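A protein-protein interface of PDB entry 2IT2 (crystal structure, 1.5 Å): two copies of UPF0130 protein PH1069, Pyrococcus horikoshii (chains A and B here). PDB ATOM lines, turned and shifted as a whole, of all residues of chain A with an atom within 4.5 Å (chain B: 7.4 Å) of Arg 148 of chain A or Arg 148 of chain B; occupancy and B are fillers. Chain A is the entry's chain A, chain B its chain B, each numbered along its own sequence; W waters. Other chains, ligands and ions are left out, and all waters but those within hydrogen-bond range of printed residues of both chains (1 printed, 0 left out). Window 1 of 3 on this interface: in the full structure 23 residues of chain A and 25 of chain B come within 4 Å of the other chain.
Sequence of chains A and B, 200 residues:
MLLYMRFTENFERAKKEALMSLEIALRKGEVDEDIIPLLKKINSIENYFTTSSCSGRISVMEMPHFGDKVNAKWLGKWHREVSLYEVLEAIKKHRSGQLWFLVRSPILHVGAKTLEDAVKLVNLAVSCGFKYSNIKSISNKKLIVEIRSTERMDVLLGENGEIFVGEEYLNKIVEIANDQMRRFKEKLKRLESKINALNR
Of the 12 printed residues of chain A, 3 touch a printed residue of chain B. Printed residues of chain A that touch a printed residue of chain B: Tyr 132, Asn 134 and Arg 148. Along chain A the printed residues that touch a printed residue of chain B span positions 132 to 148. Hydrophobic or aromatic side chains of chain B within 4 Å of the printed part of chain A: Tyr 132. Among the printed residues, no Asp or Glu carboxylate lies within 4 Å of a Lys or Arg side-chain nitrogen of the other chain.
Among the printed residues, pairs that only touch across the chains: Tyr 132 of chain A with Glu 146 of chain B (3.8 Å), Tyr 132 of chain A with Arg 148 of chain B (3.6 Å), Asn 134 of chain A with Asn 134 of chain B (3.3 Å) and Arg 148 of chain A with Tyr 132 of chain B (3.6 Å).
Water W1 lies within hydrogen-bond range of the guanidinium group (NH1) of Arg 152 of chain B and the side-chain hydroxyl (OH) of Tyr 132 of chain A.
The backbone NH (N) of Tyr 132 of chain A sits at hydrogen-bond distance from the backbone carbonyl oxygen (O) of Arg 148 of chain A. OG of Ser 133 of chain A lies within hydrogen-bond range of N of Arg 148 of chain A (3.5 Å). The backbone carbonyl oxygen (O) of Asn 134 of chain A lies within hydrogen-bond range of the backbone NH (N) of Glu 146 of chain A (2.9 Å). The side-chain amide nitrogen (ND2) of Asn 134 of chain B sits at hydrogen-bond distance from the backbone carbonyl oxygen (O) of Tyr 132 of chain B (3.5 Å). The side-chain hydroxyl (OG) of Ser 133 of chain B lies within hydrogen-bond range of the backbone NH (N) of Arg 148 of chain B. The backbone NH (N) of Glu 146 of chain B is in hydrogen-bond range of the backbone carbonyl oxygen (O) of Asn 134 of chain B, 2.9 Å away.
Of the printed residues of chain B, Tyr 132 of chain A touches Glu 146 (3.8 Å) and Arg 148 (3.6 Å). Of the printed residues of chain B, Asn 134 of chain A touches Asn 134 (3.3 Å). Of the printed residues of chain B, Arg 148 of chain A touches Tyr 132 and Arg 148. Printed residues of chain A within 4 Å of Tyr 132 of chain B: Arg 148. Printed residues of chain A within 4 Å of Asn 134 of chain B: Asn 134. Of the printed residues of chain A, Glu 146 of chain B touches Tyr 132 (3.8 Å). Arg 148 of chain B touches just these residues of chain A: Tyr 132 (3.6 Å) and Arg 148 (3.1 Å). The nearest printed residue of chain A that does not touch Tyr 132 of chain B is Glu 146 of chain A (6.1 Å).
Tyr 132 of chain A touches Glu 146 of chain B, but with the chains exchanged Glu 146 of chain A does not touch Tyr 132 of chain B (6.1 Å). Tyr 132 of chain A touches Arg 148 of chain B, and with the chains exchanged Arg 148 of chain A touches Tyr 132 of chain B. Asn 134 of chain B touches its own counterpart, Asn 134 of chain A. Arg 148 of chain A touches its own counterpart, Arg 148 of chain B. 12 positions are printed for both chains.
NH2 of Arg 148 of chain A sits close to NH2 of Arg 148 of chain B.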
ATOM      1  N   SER A 105      19.108  19.300  -0.614  1.00  0.00           N
ATOM      2  CA  SER A 105      18.128  20.066  -1.381  1.00  0.00           C
ATOM      3  C   SER A 105      18.788  20.703  -2.600  1.00  0.00           C
ATOM      4  O   SER A 105      20.009  20.839  -2.645  1.00  0.00           O
ATOM      5  CB  SER A 105      17.541  21.173  -0.506  1.00  0.00           C
ATOM      6  OG  SER A 105      17.017  22.222  -1.305  1.00  0.00           O
ATOM      7  N   PRO A 106      17.990  21.070  -3.622  1.00  0.00           N
ATOM      8  CA  PRO A 106      18.645  21.697  -4.773  1.00  0.00           C
ATOM      9  C   PRO A 106      19.187  23.017  -4.247  1.00  0.00           C
ATOM     10  O   PRO A 106      18.666  23.551  -3.271  1.00  0.00           O
ATOM     11  CB  PRO A 106      17.501  21.882  -5.770  1.00  0.00           C
ATOM     12  CG  PRO A 106      16.261  21.902  -4.899  1.00  0.00           C
ATOM     13  CD  PRO A 106      16.556  20.856  -3.871  1.00  0.00           C
ATOM     14  N   ILE A 107      20.251  23.521  -4.857  1.00  0.00           N
ATOM     15  CA  ILE A 107      20.796  24.791  -4.424  1.00  0.00           C
ATOM     16  C   ILE A 107      21.160  25.638  -5.631  1.00  0.00           C
ATOM     17  O   ILE A 107      21.788  25.180  -6.577  1.00  0.00           O
ATOM     18  CB  ILE A 107      22.045  24.513  -3.586  1.00  0.00           C
ATOM     19  CG1 ILE A 107      22.615  25.823  -3.034  1.00  0.00           C
ATOM     20  CG2 ILE A 107      23.128  23.863  -4.466  1.00  0.00           C
ATOM     21  CD1 ILE A 107      21.537  26.709  -2.407  1.00  0.00           C
ATOM     22  N   PHE A 130      11.330  27.556  -0.445  1.00  0.00           N
ATOM     23  CA  PHE A 130      12.767  27.485  -0.232  1.00  0.00           C
ATOM     24  C   PHE A 130      13.069  28.408   0.930  1.00  0.00           C
ATOM     25  O   PHE A 130      13.586  29.507   0.754  1.00  0.00           O
ATOM     26  CB  PHE A 130      13.504  27.915  -1.507  1.00  0.00           C
ATOM     27  CG  PHE A 130      13.262  26.996  -2.676  1.00  0.00           C
ATOM     28  CD1 PHE A 130      12.148  27.166  -3.497  1.00  0.00           C
ATOM     29  CD2 PHE A 130      14.130  25.937  -2.931  1.00  0.00           C
ATOM     30  CE1 PHE A 130      11.898  26.284  -4.560  1.00  0.00           C
ATOM     31  CE2 PHE A 130      13.894  25.048  -3.989  1.00  0.00           C
ATOM     32  CZ  PHE A 130      12.775  25.224  -4.804  1.00  0.00           C
ATOM     33  N   LYS A 131      12.727  27.937   2.126  1.00  0.00           N
ATOM     34  CA  LYS A 131      12.882  28.707   3.354  1.00  0.00           C
ATOM     35  C   LYS A 131      14.282  29.142   3.753  1.00  0.00           C
ATOM     36  O   LYS A 131      14.438  30.118   4.488  1.00  0.00           O
ATOM     37  CB  LYS A 131      12.246  27.939   4.509  1.00  0.00           C
ATOM     38  CG  LYS A 131      10.798  27.550   4.255  1.00  0.00           C
ATOM     39  CD  LYS A 131       9.945  28.742   3.843  1.00  0.00           C
ATOM     40  CE  LYS A 131       8.504  28.322   3.609  1.00  0.00           C
ATOM     41  NZ  LYS A 131       7.639  29.464   3.221  1.00  0.00           N
ATOM     42  N   TYR A 132      15.301  28.424   3.298  1.00  0.00           N
ATOM     43  CA  TYR A 132      16.662  28.799   3.645  1.00  0.00           C
ATOM     44  C   TYR A 132      17.334  29.693   2.623  1.00  0.00           C
ATOM     45  O   TYR A 132      18.557  29.792   2.607  1.00  0.00           O
ATOM     46  CB  TYR A 132      17.527  27.563   3.857  1.00  0.00           C
ATOM     47  CG  TYR A 132      17.521  27.086   5.282  1.00  0.00           C
ATOM     48  CD1 TYR A 132      17.894  27.944   6.316  1.00  0.00           C
ATOM     49  CD2 TYR A 132      17.146  25.785   5.602  1.00  0.00           C
ATOM     50  CE1 TYR A 132      17.892  27.521   7.639  1.00  0.00           C
ATOM     51  CE2 TYR A 132      17.140  25.346   6.931  1.00  0.00           C
ATOM     52  CZ  TYR A 132      17.517  26.224   7.942  1.00  0.00           C
ATOM     53  OH  TYR A 132      17.525  25.810   9.254  1.00  0.00           O
ATOM     54  N   SER A 133      16.541  30.334   1.771  1.00  0.00           N
ATOM     55  CA  SER A 133      17.085  31.233   0.754  1.00  0.00           C
ATOM     56  C   SER A 133      17.624  32.441   1.511  1.00  0.00           C
ATOM     57  O   SER A 133      17.058  32.856   2.525  1.00  0.00           O
ATOM     58  CB  SER A 133      15.991  31.612  -0.249  1.00  0.00           C
ATOM     59  OG  SER A 133      15.504  30.446  -0.899  1.00  0.00           O
ATOM     60  N   ASN A 134      18.712  33.017   1.019  1.00  0.00           N
ATOM     61  CA  ASN A 134      19.349  34.112   1.734  1.00  0.00           C
ATOM     62  C   ASN A 134      20.317  34.862   0.837  1.00  0.00           C
ATOM     63  O   ASN A 134      20.477  34.548  -0.338  1.00  0.00           O
ATOM     64  CB  ASN A 134      20.166  33.508   2.867  1.00  0.00           C
ATOM     65  CG  ASN A 134      21.215  32.547   2.340  1.00  0.00           C
ATOM     66  OD1 ASN A 134      22.356  32.932   2.070  1.00  0.00           O
ATOM     67  ND2 ASN A 134      20.853  31.276   2.244  1.00  0.00           N
ATOM     68  N   GLU A 146      21.357  32.958  -2.550  1.00  0.00           N
ATOM     69  CA  GLU A 146      21.380  31.501  -2.514  1.00  0.00           C
ATOM     70  C   GLU A 146      19.945  31.052  -2.288  1.00  0.00           C
ATOM     71  O   GLU A 146      19.260  31.575  -1.412  1.00  0.00           O
ATOM     72  CB  GLU A 146      22.257  30.976  -1.372  1.00  0.00           C
ATOM     73  CG  GLU A 146      22.369  29.467  -1.374  1.00  0.00           C
ATOM     74  CD  GLU A 146      23.298  28.945  -0.311  1.00  0.00           C
ATOM     75  OE1 GLU A 146      22.935  28.997   0.885  1.00  0.00           O
ATOM     76  OE2 GLU A 146      24.396  28.484  -0.675  1.00  0.00           O
ATOM     77  N   ILE A 147      19.488  30.109  -3.098  1.00  0.00           N
ATOM     78  CA  ILE A 147      18.134  29.576  -2.976  1.00  0.00           C
ATOM     79  C   ILE A 147      18.290  28.136  -2.500  1.00  0.00           C
ATOM     80  O   ILE A 147      18.963  27.340  -3.146  1.00  0.00           O
ATOM     81  CB  ILE A 147      17.397  29.615  -4.339  1.00  0.00           C
ATOM     82  CG1 ILE A 147      17.226  31.073  -4.787  1.00  0.00           C
ATOM     83  CG2 ILE A 147      16.031  28.922  -4.226  1.00  0.00           C
ATOM     84  CD1 ILE A 147      16.558  31.252  -6.146  1.00  0.00           C
ATOM     85  N   ARG A 148      17.676  27.806  -1.366  1.00  0.00           N
ATOM     86  CA  ARG A 148      17.794  26.464  -0.809  1.00  0.00           C
ATOM     87  C   ARG A 148      16.580  26.099   0.035  1.00  0.00           C
ATOM     88  O   ARG A 148      16.000  26.956   0.702  1.00  0.00           O
ATOM     89  CB  ARG A 148      19.062  26.379   0.045  1.00  0.00           C
ATOM     90  CG  ARG A 148      19.283  25.039   0.712  1.00  0.00           C
ATOM     91  CD  ARG A 148      20.441  25.114   1.683  1.00  0.00           C
ATOM     92  NE  ARG A 148      20.249  26.189   2.653  1.00  0.00           N
ATOM     93  CZ  ARG A 148      21.065  26.433   3.672  1.00  0.00           C
ATOM     94  NH1 ARG A 148      22.140  25.676   3.863  1.00  0.00           N
ATOM     95  NH2 ARG A 148      20.807  27.432   4.507  1.00  0.00           N
ATOM     96  N   SER A 149      16.213  24.818   0.012  1.00  0.00           N
ATOM     97  CA  SER A 149      15.065  24.323   0.763  1.00  0.00           C
ATOM     98  C   SER A 149      15.483  23.733   2.116  1.00  0.00           C
ATOM     99  O   SER A 149      16.646  23.829   2.511  1.00  0.00           O
ATOM    100  CB  SER A 149      14.321  23.276  -0.071  1.00  0.00           C
ATOM    101  OG  SER A 149      13.043  23.000   0.469  1.00  0.00           O
ATOM    102  N   ARG B 104      20.394  19.082  16.085  1.00  0.00           N
ATOM    103  CA  ARG B 104      20.325  20.347  15.351  1.00  0.00           C
ATOM    104  C   ARG B 104      21.279  21.391  15.911  1.00  0.00           C
ATOM    105  O   ARG B 104      21.462  21.502  17.123  1.00  0.00           O
ATOM    106  CB  ARG B 104      18.901  20.908  15.374  1.00  0.00           C
ATOM    107  CG  ARG B 104      17.903  20.052  14.622  1.00  0.00           C
ATOM    108  CD  ARG B 104      18.178  20.081  13.126  1.00  0.00           C
ATOM    109  NE  ARG B 104      17.177  19.337  12.365  1.00  0.00           N
ATOM    110  CZ  ARG B 104      17.230  18.030  12.132  1.00  0.00           C
ATOM    111  NH1 ARG B 104      18.241  17.317  12.601  1.00  0.00           N
ATOM    112  NH2 ARG B 104      16.264  17.436  11.436  1.00  0.00           N
ATOM    113  N   SER B 105      21.859  22.167  15.001  1.00  0.00           N
ATOM    114  CA  SER B 105      22.815  23.223  15.341  1.00  0.00           C
ATOM    115  C   SER B 105      22.190  24.408  16.055  1.00  0.00           C
ATOM    116  O   SER B 105      20.984  24.644  15.944  1.00  0.00           O
ATOM    117  CB  SER B 105      23.486  23.735  14.059  1.00  0.00           C
ATOM    118  OG  SER B 105      24.033  25.037  14.251  1.00  0.00           O
ATOM    119  N   PRO B 106      23.002  25.154  16.824  1.00  0.00           N
ATOM    120  CA  PRO B 106      22.451  26.322  17.509  1.00  0.00           C
ATOM    121  C   PRO B 106      22.094  27.295  16.374  1.00  0.00           C
ATOM    122  O   PRO B 106      22.660  27.213  15.271  1.00  0.00           O
ATOM    123  CB  PRO B 106      23.636  26.847  18.337  1.00  0.00           C
ATOM    124  CG  PRO B 106      24.470  25.650  18.577  1.00  0.00           C
ATOM    125  CD  PRO B 106      24.380  24.879  17.269  1.00  0.00           C
ATOM    126  N   ILE B 107      21.153  28.193  16.644  1.00  0.00           N
ATOM    127  CA  ILE B 107      20.752  29.200  15.671  1.00  0.00           C
ATOM    128  C   ILE B 107      20.656  30.540  16.389  1.00  0.00           C
ATOM    129  O   ILE B 107      19.942  30.674  17.383  1.00  0.00           O
ATOM    130  CB  ILE B 107      19.371  28.902  15.050  1.00  0.00           C
ATOM    131  CG1 ILE B 107      19.387  27.555  14.327  1.00  0.00           C
ATOM    132  CG2 ILE B 107      18.994  30.035  14.093  1.00  0.00           C
ATOM    133  CD1 ILE B 107      18.060  27.178  13.707  1.00  0.00           C
ATOM    134  N   LEU B 108      21.387  31.531  15.893  1.00  0.00           N
ATOM    135  CA  LEU B 108      21.347  32.856  16.499  1.00  0.00           C
ATOM    136  C   LEU B 108      20.829  33.833  15.441  1.00  0.00           C
ATOM    137  O   LEU B 108      21.206  33.753  14.261  1.00  0.00           O
ATOM    138  CB  LEU B 108      22.753  33.283  16.969  1.00  0.00           C
ATOM    139  CG  LEU B 108      23.619  32.302  17.780  1.00  0.00           C
ATOM    140  CD1 LEU B 108      25.003  32.896  17.994  1.00  0.00           C
ATOM    141  CD2 LEU B 108      22.958  31.980  19.122  1.00  0.00           C
ATOM    142  N   ALA B 125      31.440  34.981  11.895  1.00  0.00           N
ATOM    143  CA  ALA B 125      30.775  33.760  12.328  1.00  0.00           C
ATOM    144  C   ALA B 125      31.297  32.562  11.540  1.00  0.00           C
ATOM    145  O   ALA B 125      31.622  31.526  12.119  1.00  0.00           O
ATOM    146  CB  ALA B 125      29.271  33.905  12.164  1.00  0.00           C
ATOM    147  N   VAL B 126      31.397  32.713  10.221  1.00  0.00           N
ATOM    148  CA  VAL B 126      31.901  31.624   9.392  1.00  0.00           C
ATOM    149  C   VAL B 126      33.297  31.198   9.845  1.00  0.00           C
ATOM    150  O   VAL B 126      33.621  30.011   9.861  1.00  0.00           O
ATOM    151  CB  VAL B 126      31.955  32.035   7.908  1.00  0.00           C
ATOM    152  CG1 VAL B 126      32.695  30.976   7.095  1.00  0.00           C
ATOM    153  CG2 VAL B 126      30.544  32.218   7.373  1.00  0.00           C
ATOM    154  N   GLY B 129      33.406  28.744  12.733  1.00  0.00           N
ATOM    155  CA  GLY B 129      32.839  27.420  12.548  1.00  0.00           C
ATOM    156  C   GLY B 129      31.364  27.366  12.212  1.00  0.00           C
ATOM    157  O   GLY B 129      30.782  26.285  12.185  1.00  0.00           O
ATOM    158  N   PHE B 130      30.750  28.513  11.947  1.00  0.00           N
ATOM    159  CA  PHE B 130      29.330  28.532  11.612  1.00  0.00           C
ATOM    160  C   PHE B 130      29.225  28.821  10.114  1.00  0.00           C
ATOM    161  O   PHE B 130      28.919  29.929   9.686  1.00  0.00           O
ATOM    162  CB  PHE B 130      28.601  29.590  12.460  1.00  0.00           C
ATOM    163  CG  PHE B 130      28.587  29.285  13.949  1.00  0.00           C
ATOM    164  CD1 PHE B 130      27.633  28.426  14.493  1.00  0.00           C
ATOM    165  CD2 PHE B 130      29.516  29.868  14.802  1.00  0.00           C
ATOM    166  CE1 PHE B 130      27.607  28.159  15.878  1.00  0.00           C
ATOM    167  CE2 PHE B 130      29.500  29.610  16.174  1.00  0.00           C
ATOM    168  CZ  PHE B 130      28.543  28.756  16.715  1.00  0.00           C
ATOM    169  N   LYS B 131      29.479  27.791   9.316  1.00  0.00           N
ATOM    170  CA  LYS B 131      29.472  27.937   7.869  1.00  0.00           C
ATOM    171  C   LYS B 131      28.144  28.346   7.258  1.00  0.00           C
ATOM    172  O   LYS B 131      28.113  28.978   6.194  1.00  0.00           O
ATOM    173  CB  LYS B 131      29.978  26.647   7.224  1.00  0.00           C
ATOM    174  CG  LYS B 131      31.481  26.480   7.325  1.00  0.00           C
ATOM    175  CD  LYS B 131      32.185  27.555   6.508  1.00  0.00           C
ATOM    176  CE  LYS B 131      33.701  27.406   6.544  1.00  0.00           C
ATOM    177  NZ  LYS B 131      34.391  28.441   5.712  1.00  0.00           N
ATOM    178  N   TYR B 132      27.042  28.006   7.915  1.00  0.00           N
ATOM    179  CA  TYR B 132      25.737  28.367   7.379  1.00  0.00           C
ATOM    180  C   TYR B 132      25.245  29.733   7.854  1.00  0.00           C
ATOM    181  O   TYR B 132      24.055  29.929   8.091  1.00  0.00           O
ATOM    182  CB  TYR B 132      24.696  27.286   7.703  1.00  0.00           C
ATOM    183  CG  TYR B 132      24.870  25.997   6.925  1.00  0.00           C
ATOM    184  CD1 TYR B 132      25.334  26.008   5.609  1.00  0.00           C
ATOM    185  CD2 TYR B 132      24.513  24.769   7.486  1.00  0.00           C
ATOM    186  CE1 TYR B 132      25.440  24.827   4.869  1.00  0.00           C
ATOM    187  CE2 TYR B 132      24.611  23.585   6.756  1.00  0.00           C
ATOM    188  CZ  TYR B 132      25.072  23.621   5.450  1.00  0.00           C
ATOM    189  OH  TYR B 132      25.151  22.456   4.720  1.00  0.00           O
ATOM    190  N   SER B 133      26.158  30.687   7.987  1.00  0.00           N
ATOM    191  CA  SER B 133      25.767  32.017   8.417  1.00  0.00           C
ATOM    192  C   SER B 133      25.530  32.898   7.195  1.00  0.00           C
ATOM    193  O   SER B 133      26.247  32.786   6.190  1.00  0.00           O
ATOM    194  CB  SER B 133      26.845  32.614   9.324  1.00  0.00           C
ATOM    195  OG  SER B 133      27.015  31.814  10.493  1.00  0.00           O
ATOM    196  N   ASN B 134      24.542  33.783   7.279  1.00  0.00           N
ATOM    197  CA  ASN B 134      24.225  34.636   6.135  1.00  0.00           C
ATOM    198  C   ASN B 134      23.241  35.740   6.501  1.00  0.00           C
ATOM    199  O   ASN B 134      22.934  35.930   7.669  1.00  0.00           O
ATOM    200  CB  ASN B 134      23.626  33.764   5.027  1.00  0.00           C
ATOM    201  CG  ASN B 134      22.551  32.823   5.546  1.00  0.00           C
ATOM    202  OD1 ASN B 134      21.578  33.252   6.170  1.00  0.00           O
ATOM    203  ND2 ASN B 134      22.726  31.525   5.293  1.00  0.00           N
ATOM    204  N   GLU B 146      21.675  35.445  10.286  1.00  0.00           N
ATOM    205  CA  GLU B 146      21.442  34.147  10.936  1.00  0.00           C
ATOM    206  C   GLU B 146      22.788  33.450  11.016  1.00  0.00           C
ATOM    207  O   GLU B 146      23.527  33.410  10.030  1.00  0.00           O
ATOM    208  CB  GLU B 146      20.477  33.280  10.122  1.00  0.00           C
ATOM    209  CG  GLU B 146      20.170  31.918  10.733  1.00  0.00           C
ATOM    210  CD  GLU B 146      19.061  31.215   9.984  1.00  0.00           C
ATOM    211  OE1 GLU B 146      19.295  30.799   8.830  1.00  0.00           O
ATOM    212  OE2 GLU B 146      17.950  31.090  10.541  1.00  0.00           O
ATOM    213  N   ILE B 147      23.108  32.923  12.198  1.00  0.00           N
ATOM    214  CA  ILE B 147      24.360  32.203  12.452  1.00  0.00           C
ATOM    215  C   ILE B 147      23.975  30.750  12.730  1.00  0.00           C
ATOM    216  O   ILE B 147      23.157  30.473  13.611  1.00  0.00           O
ATOM    217  CB  ILE B 147      25.089  32.812  13.668  1.00  0.00           C
ATOM    218  CG1 ILE B 147      25.459  34.267  13.359  1.00  0.00           C
ATOM    219  CG2 ILE B 147      26.320  31.982  14.035  1.00  0.00           C
ATOM    220  CD1 ILE B 147      26.090  34.999  14.522  1.00  0.00           C
ATOM    221  N   ARG B 148      24.557  29.825  11.976  1.00  0.00           N
ATOM    222  CA  ARG B 148      24.218  28.413  12.113  1.00  0.00           C
ATOM    223  C   ARG B 148      25.368  27.544  11.622  1.00  0.00           C
ATOM    224  O   ARG B 148      26.125  27.955  10.741  1.00  0.00           O
ATOM    225  CB  ARG B 148      22.951  28.146  11.293  1.00  0.00           C
ATOM    226  CG  ARG B 148      22.323  26.780  11.470  1.00  0.00           C
ATOM    227  CD  ARG B 148      20.945  26.749  10.816  1.00  0.00           C
ATOM    228  NE  ARG B 148      21.015  26.873   9.363  1.00  0.00           N
ATOM    229  CZ  ARG B 148      21.318  25.881   8.530  1.00  0.00           C
ATOM    230  NH1 ARG B 148      21.587  24.663   8.989  1.00  0.00           N
ATOM    231  NH2 ARG B 148      21.359  26.114   7.225  1.00  0.00           N
ATOM    232  N   SER B 149      25.487  26.344  12.191  1.00  0.00           N
ATOM    233  CA  SER B 149      26.539  25.393  11.831  1.00  0.00           C
ATOM    234  C   SER B 149      25.968  24.302  10.924  1.00  0.00           C
ATOM    235  O   SER B 149      24.749  24.155  10.806  1.00  0.00           O
ATOM    236  CB  SER B 149      27.140  24.767  13.101  1.00  0.00           C
ATOM    237  OG  SER B 149      28.403  24.165  12.840  1.00  0.00           O
ATOM    238  N   THR B 150      26.856  23.534  10.297  1.00  0.00           N
ATOM    239  CA  THR B 150      26.459  22.474   9.368  1.00  0.00           C
ATOM    240  C   THR B 150      26.159  21.109   9.973  1.00  0.00           C
ATOM    241  O   THR B 150      25.465  20.302   9.352  1.00  0.00           O
ATOM    242  CB  THR B 150      27.536  22.252   8.304  1.00  0.00           C
ATOM    243  OG1 THR B 150      28.713  21.717   8.929  1.00  0.00           O
ATOM    244  CG2 THR B 150      27.867  23.563   7.609  1.00  0.00           C
ATOM    245  N   GLU B 151      26.691  20.839  11.161  1.00  0.00           N
ATOM    246  CA  GLU B 151      26.491  19.548  11.821  1.00  0.00           C
ATOM    247  C   GLU B 151      25.041  19.237  12.154  1.00  0.00           C
ATOM    248  O   GLU B 151      24.295  20.100  12.614  1.00  0.00           O
ATOM    249  CB  GLU B 151      27.322  19.475  13.106  1.00  0.00           C
ATOM    250  CG  GLU B 151      28.820  19.333  12.874  1.00  0.00           C
ATOM    251  CD  GLU B 151      29.348  20.315  11.844  1.00  0.00           C
ATOM    252  OE1 GLU B 151      29.195  21.538  12.051  1.00  0.00           O
ATOM    253  OE2 GLU B 151      29.914  19.865  10.823  1.00  0.00           O
ATOM    254  N   ARG B 152      24.647  17.992  11.914  1.00  0.00           N
ATOM    255  CA  ARG B 152      23.291  17.552  12.221  1.00  0.00           C
ATOM    256  C   ARG B 152      23.183  16.049  12.027  1.00  0.00           C
ATOM    257  O   ARG B 152      24.069  15.419  11.444  1.00  0.00           O
ATOM    258  CB  ARG B 152      22.276  18.249  11.318  1.00  0.00           C
ATOM    259  CG  ARG B 152      22.403  17.879   9.853  1.00  0.00           C
ATOM    260  CD  ARG B 152      21.356  18.598   9.004  1.00  0.00           C
ATOM    261  NE  ARG B 152      20.005  18.107   9.260  1.00  0.00           N
ATOM    262  CZ  ARG B 152      18.896  18.700   8.825  1.00  0.00           C
ATOM    263  NH1 ARG B 152      18.975  19.813   8.110  1.00  0.00           N
ATOM    264  NH2 ARG B 152      17.707  18.176   9.092  1.00  0.00           N
ATOM    265  N   PHE B 184      29.286  22.090  18.974  1.00  0.00           N
ATOM    266  CA  PHE B 184      28.442  23.282  18.969  1.00  0.00           C
ATOM    267  C   PHE B 184      28.825  24.194  20.129  1.00  0.00           C
ATOM    268  O   PHE B 184      28.973  25.409  19.961  1.00  0.00           O
ATOM    269  CB  PHE B 184      26.965  22.911  19.127  1.00  0.00           C
ATOM    270  CG  PHE B 184      26.400  22.113  17.987  1.00  0.00           C
ATOM    271  CD1 PHE B 184      26.824  22.325  16.681  1.00  0.00           C
ATOM    272  CD2 PHE B 184      25.396  21.174  18.218  1.00  0.00           C
ATOM    273  CE1 PHE B 184      26.250  21.622  15.616  1.00  0.00           C
ATOM    274  CE2 PHE B 184      24.819  20.470  17.160  1.00  0.00           C
ATOM    275  CZ  PHE B 184      25.248  20.692  15.866  1.00  0.00           C
ATOM    276  N   LYS B 187      32.169  25.936  19.513  1.00  0.00           N
ATOM    277  CA  LYS B 187      32.037  27.004  18.528  1.00  0.00           C
ATOM    278  C   LYS B 187      31.353  28.241  19.113  1.00  0.00           C
ATOM    279  O   LYS B 187      31.701  29.372  18.769  1.00  0.00           O
ATOM    280  CB  LYS B 187      31.264  26.498  17.304  1.00  0.00           C
ATOM    281  CG  LYS B 187      32.042  25.473  16.495  1.00  0.00           C
ATOM    282  CD  LYS B 187      31.276  25.016  15.271  1.00  0.00           C
ATOM    283  CE  LYS B 187      32.142  24.083  14.438  1.00  0.00           C
ATOM    284  NZ  LYS B 187      31.409  23.632  13.232  1.00  0.00           N
HETATM  285  O   HOH W   1      18.198  22.536   9.965  1.00  0.00           O
